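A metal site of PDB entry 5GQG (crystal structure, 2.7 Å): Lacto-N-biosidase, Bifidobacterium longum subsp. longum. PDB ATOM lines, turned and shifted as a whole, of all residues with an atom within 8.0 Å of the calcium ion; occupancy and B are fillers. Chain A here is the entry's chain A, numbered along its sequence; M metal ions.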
ATOM      1  N   ASN A 148       6.746   7.179 -15.128  1.00  0.00           N
ATOM      2  CA  ASN A 148       7.730   7.325 -14.078  1.00  0.00           C
ATOM      3  C   ASN A 148       9.066   7.379 -14.743  1.00  0.00           C
ATOM      4  O   ASN A 148       9.910   6.510 -14.574  1.00  0.00           O
ATOM      5  CB  ASN A 148       7.659   6.209 -13.039  1.00  0.00           C
ATOM      6  CG  ASN A 148       8.355   6.600 -11.754  1.00  0.00           C
ATOM      7  OD1 ASN A 148       9.203   7.516 -11.755  1.00  0.00           O
ATOM      8  ND2 ASN A 148       7.996   5.954 -10.635  1.00  0.00           N
ATOM      9  N   ASP A 149       9.234   8.452 -15.495  1.00  0.00           N
ATOM     10  CA  ASP A 149      10.268   8.569 -16.483  1.00  0.00           C
ATOM     11  C   ASP A 149      11.524   9.172 -15.894  1.00  0.00           C
ATOM     12  O   ASP A 149      11.464  10.143 -15.159  1.00  0.00           O
ATOM     13  CB  ASP A 149       9.754   9.478 -17.590  1.00  0.00           C
ATOM     14  CG  ASP A 149      10.678   9.564 -18.732  1.00  0.00           C
ATOM     15  OD1 ASP A 149      11.014   8.504 -19.264  1.00  0.00           O
ATOM     16  OD2 ASP A 149      11.106  10.664 -19.113  1.00  0.00           O
ATOM     17  N   ASP A 150      12.656   8.557 -16.196  1.00  0.00           N
ATOM     18  CA  ASP A 150      13.963   9.186 -16.112  1.00  0.00           C
ATOM     19  C   ASP A 150      14.215   9.819 -17.488  1.00  0.00           C
ATOM     20  O   ASP A 150      13.933   9.205 -18.517  1.00  0.00           O
ATOM     21  CB  ASP A 150      15.058   8.143 -15.817  1.00  0.00           C
ATOM     22  CG  ASP A 150      16.323   8.724 -15.121  1.00  0.00           C
ATOM     23  OD1 ASP A 150      16.698   9.898 -15.322  1.00  0.00           O
ATOM     24  OD2 ASP A 150      16.964   7.955 -14.378  1.00  0.00           O
ATOM     25  N   ALA A 151      14.695  11.053 -17.487  1.00  0.00           N
ATOM     26  CA  ALA A 151      15.042  11.771 -18.685  1.00  0.00           C
ATOM     27  C   ALA A 151      16.386  11.318 -19.173  1.00  0.00           C
ATOM     28  O   ALA A 151      16.693  11.475 -20.350  1.00  0.00           O
ATOM     29  CB  ALA A 151      15.074  13.261 -18.411  1.00  0.00           C
ATOM     30  N   ASP A 152      17.195  10.791 -18.249  1.00  0.00           N
ATOM     31  CA  ASP A 152      18.539  10.259 -18.548  1.00  0.00           C
ATOM     32  C   ASP A 152      18.572   8.794 -19.002  1.00  0.00           C
ATOM     33  O   ASP A 152      19.626   8.328 -19.392  1.00  0.00           O
ATOM     34  CB  ASP A 152      19.491  10.452 -17.341  1.00  0.00           C
ATOM     35  CG  ASP A 152      20.260  11.765 -17.400  1.00  0.00           C
ATOM     36  OD1 ASP A 152      20.690  12.172 -18.521  1.00  0.00           O
ATOM     37  OD2 ASP A 152      20.435  12.375 -16.317  1.00  0.00           O
ATOM     38  N   VAL A 153      17.435   8.100 -18.943  1.00  0.00           N
ATOM     39  CA  VAL A 153      17.274   6.765 -19.548  1.00  0.00           C
ATOM     40  C   VAL A 153      16.324   6.914 -20.725  1.00  0.00           C
ATOM     41  O   VAL A 153      15.221   7.408 -20.536  1.00  0.00           O
ATOM     42  CB  VAL A 153      16.686   5.730 -18.539  1.00  0.00           C
ATOM     43  CG1 VAL A 153      16.219   4.436 -19.208  1.00  0.00           C
ATOM     44  CG2 VAL A 153      17.718   5.423 -17.459  1.00  0.00           C
ATOM     45  N   TYR A 154      16.741   6.493 -21.913  1.00  0.00           N
ATOM     46  CA  TYR A 154      15.897   6.512 -23.108  1.00  0.00           C
ATOM     47  C   TYR A 154      16.246   5.284 -23.962  1.00  0.00           C
ATOM     48  O   TYR A 154      17.386   5.170 -24.394  1.00  0.00           O
ATOM     49  CB  TYR A 154      16.144   7.821 -23.878  1.00  0.00           C
ATOM     50  CG  TYR A 154      15.367   7.964 -25.163  1.00  0.00           C
ATOM     51  CD1 TYR A 154      13.965   7.980 -25.161  1.00  0.00           C
ATOM     52  CD2 TYR A 154      16.037   8.085 -26.416  1.00  0.00           C
ATOM     53  CE1 TYR A 154      13.245   8.090 -26.357  1.00  0.00           C
ATOM     54  CE2 TYR A 154      15.330   8.214 -27.609  1.00  0.00           C
ATOM     55  CZ  TYR A 154      13.942   8.211 -27.572  1.00  0.00           C
ATOM     56  OH  TYR A 154      13.230   8.318 -28.744  1.00  0.00           O
ATOM     57  N   ASP A 155      15.312   4.362 -24.171  1.00  0.00           N
ATOM     58  CA  ASP A 155      15.555   3.186 -25.056  1.00  0.00           C
ATOM     59  C   ASP A 155      14.268   2.561 -25.611  1.00  0.00           C
ATOM     60  O   ASP A 155      13.902   1.431 -25.264  1.00  0.00           O
ATOM     61  CB  ASP A 155      16.385   2.125 -24.324  1.00  0.00           C
ATOM     62  CG  ASP A 155      16.828   0.984 -25.239  1.00  0.00           C
ATOM     63  OD1 ASP A 155      16.637   1.064 -26.476  1.00  0.00           O
ATOM     64  OD2 ASP A 155      17.390   0.008 -24.686  1.00  0.00           O
ATOM     65  N   PRO A 156      13.581   3.289 -26.500  1.00  0.00           N
ATOM     66  CA  PRO A 156      12.231   2.901 -26.842  1.00  0.00           C
ATOM     67  C   PRO A 156      12.181   1.634 -27.721  1.00  0.00           C
ATOM     68  O   PRO A 156      13.093   1.384 -28.583  1.00  0.00           O
ATOM     69  CB  PRO A 156      11.713   4.120 -27.579  1.00  0.00           C
ATOM     70  CG  PRO A 156      12.916   4.678 -28.247  1.00  0.00           C
ATOM     71  CD  PRO A 156      14.117   4.271 -27.459  1.00  0.00           C
ATOM     72  N   LYS A 172      20.289   5.323 -24.180  1.00  0.00           N
ATOM     73  CA  LYS A 172      21.082   5.419 -22.962  1.00  0.00           C
ATOM     74  C   LYS A 172      20.391   4.664 -21.825  1.00  0.00           C
ATOM     75  O   LYS A 172      19.190   4.823 -21.588  1.00  0.00           O
ATOM     76  CB  LYS A 172      21.252   6.891 -22.577  1.00  0.00           C
ATOM     77  CG  LYS A 172      22.517   7.191 -21.778  1.00  0.00           C
ATOM     78  CD  LYS A 172      22.355   8.534 -21.043  1.00  0.00           C
ATOM     79  CE  LYS A 172      23.663   9.156 -20.565  1.00  0.00           C
ATOM     80  NZ  LYS A 172      23.613  10.645 -20.676  1.00  0.00           N
ATOM     81  N   ARG A 179      20.379   0.966  -8.861  1.00  0.00           N
ATOM     82  CA  ARG A 179      19.402   1.911  -9.349  1.00  0.00           C
ATOM     83  C   ARG A 179      18.103   1.764  -8.608  1.00  0.00           C
ATOM     84  O   ARG A 179      17.732   0.647  -8.180  1.00  0.00           O
ATOM     85  CB  ARG A 179      19.138   1.683 -10.844  1.00  0.00           C
ATOM     86  CG  ARG A 179      18.119   2.643 -11.437  1.00  0.00           C
ATOM     87  CD  ARG A 179      17.883   2.435 -12.904  1.00  0.00           C
ATOM     88  NE  ARG A 179      16.826   3.369 -13.279  1.00  0.00           N
ATOM     89  CZ  ARG A 179      16.985   4.668 -13.533  1.00  0.00           C
ATOM     90  NH1 ARG A 179      18.183   5.240 -13.498  1.00  0.00           N
ATOM     91  NH2 ARG A 179      15.930   5.408 -13.838  1.00  0.00           N
ATOM     92  N   ARG A 182      11.291   1.457  -9.673  1.00  0.00           N
ATOM     93  CA  ARG A 182      10.168   2.334 -10.032  1.00  0.00           C
ATOM     94  C   ARG A 182       8.952   1.577 -10.511  1.00  0.00           C
ATOM     95  O   ARG A 182       9.061   0.654 -11.318  1.00  0.00           O
ATOM     96  CB  ARG A 182      10.540   3.313 -11.140  1.00  0.00           C
ATOM     97  CG  ARG A 182      11.718   4.195 -10.811  1.00  0.00           C
ATOM     98  CD  ARG A 182      11.667   5.468 -11.640  1.00  0.00           C
ATOM     99  NE  ARG A 182      12.945   6.184 -11.744  1.00  0.00           N
ATOM    100  CZ  ARG A 182      13.081   7.438 -12.180  1.00  0.00           C
ATOM    101  NH1 ARG A 182      12.017   8.168 -12.569  1.00  0.00           N
ATOM    102  NH2 ARG A 182      14.291   7.987 -12.234  1.00  0.00           N
ATOM    103  N   HIS A 206       3.490   3.884 -19.115  1.00  0.00           N
ATOM    104  CA  HIS A 206       4.626   3.839 -20.028  1.00  0.00           C
ATOM    105  C   HIS A 206       5.824   4.697 -19.579  1.00  0.00           C
ATOM    106  O   HIS A 206       5.701   5.564 -18.722  1.00  0.00           O
ATOM    107  CB  HIS A 206       4.182   4.206 -21.459  1.00  0.00           C
ATOM    108  CG  HIS A 206       3.943   5.677 -21.673  1.00  0.00           C
ATOM    109  ND1 HIS A 206       4.954   6.532 -22.042  1.00  0.00           N
ATOM    110  CD2 HIS A 206       2.833   6.423 -21.536  1.00  0.00           C
ATOM    111  CE1 HIS A 206       4.476   7.769 -22.125  1.00  0.00           C
ATOM    112  NE2 HIS A 206       3.190   7.722 -21.820  1.00  0.00           N
ATOM    113  N   ASP A 207       6.974   4.454 -20.170  1.00  0.00           N
ATOM    114  CA  ASP A 207       8.217   5.072 -19.709  1.00  0.00           C
ATOM    115  C   ASP A 207       8.368   5.064 -18.154  1.00  0.00           C
ATOM    116  O   ASP A 207       8.429   6.117 -17.524  1.00  0.00           O
ATOM    117  CB  ASP A 207       8.333   6.468 -20.311  1.00  0.00           C
ATOM    118  CG  ASP A 207       8.541   6.406 -21.808  1.00  0.00           C
ATOM    119  OD1 ASP A 207       9.707   6.204 -22.229  1.00  0.00           O
ATOM    120  OD2 ASP A 207       7.545   6.553 -22.551  1.00  0.00           O
ATOM    121  N   VAL A 208       8.388   3.852 -17.584  1.00  0.00           N
ATOM    122  CA  VAL A 208       8.645   3.557 -16.145  1.00  0.00           C
ATOM    123  C   VAL A 208      10.054   2.994 -16.061  1.00  0.00           C
ATOM    124  O   VAL A 208      10.254   1.771 -16.137  1.00  0.00           O
ATOM    125  CB  VAL A 208       7.620   2.543 -15.535  1.00  0.00           C
ATOM    126  CG1 VAL A 208       8.046   1.992 -14.164  1.00  0.00           C
ATOM    127  CG2 VAL A 208       6.213   3.173 -15.454  1.00  0.00           C
ATOM    128  N   ASP A 209      11.032   3.884 -15.901  1.00  0.00           N
ATOM    129  CA  ASP A 209      12.449   3.533 -15.876  1.00  0.00           C
ATOM    130  C   ASP A 209      12.913   3.030 -14.486  1.00  0.00           C
ATOM    131  O   ASP A 209      13.602   3.721 -13.744  1.00  0.00           O
ATOM    132  CB  ASP A 209      13.286   4.731 -16.316  1.00  0.00           C
ATOM    133  CG  ASP A 209      12.908   5.247 -17.703  1.00  0.00           C
ATOM    134  OD1 ASP A 209      12.599   4.446 -18.607  1.00  0.00           O
ATOM    135  OD2 ASP A 209      12.929   6.485 -17.879  1.00  0.00           O
ATOM    136  N   ASP A 260       7.331   0.258 -22.704  1.00  0.00           N
ATOM    137  CA  ASP A 260       8.628   0.841 -22.280  1.00  0.00           C
ATOM    138  C   ASP A 260       8.826   0.991 -20.759  1.00  0.00           C
ATOM    139  O   ASP A 260       8.923   2.103 -20.225  1.00  0.00           O
ATOM    140  CB  ASP A 260       8.862   2.194 -22.962  1.00  0.00           C
ATOM    141  CG  ASP A 260       9.246   2.084 -24.430  1.00  0.00           C
ATOM    142  OD1 ASP A 260       9.994   1.172 -24.824  1.00  0.00           O
ATOM    143  OD2 ASP A 260       8.803   2.969 -25.195  1.00  0.00           O
HETATM  144 CA    CA M   1      13.037   7.842 -20.213  1.00  0.00          CA
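O of Asp 207 lies within hydrogen-bond range of N of Asp 149, 3.2 Å away.
The guanidinium group of Arg 182 sits at hydrogen-bond distance from the backbone carbonyl oxygen of Asp 149, 3.3 Å away.
N of Asp 152 sits at hydrogen-bond distance from OD1 of Asp 150 (3.1 Å).
The guanidinium group (NH2) of Arg 179 lies within salt-bridge range of the side-chain carboxylate (OD2) of Asp 150 (2.8 Å).
OD2 of Asp 150 is in salt-bridge range of NH2 of Arg 182, at 3.4 Å.
N of Asp 209 lies within hydrogen-bond range of O of Asn 148 (3.1 Å).
O of Asp 209 is in hydrogen-bond range of NH2 of Arg 179 (2.9 Å).
The backbone carbonyl oxygen of Asp 209 is in hydrogen-bond range of the guanidinium group of Arg 182 (3.2 Å).
Of the 17 residues printed, 4 come within 4 Å of the calcium ion.
The calcium ion is bound by the backbone carbonyl oxygen of Val 153 (2.3 Å), the side-chain carboxylate of Asp 149 (2.3 Å), the backbone carbonyl oxygen of Asp 150 (2.4 Å) and the side-chain carboxylate of Asp 209 (2.7 Å).
The calcium ion has four donor atoms within binding distance.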
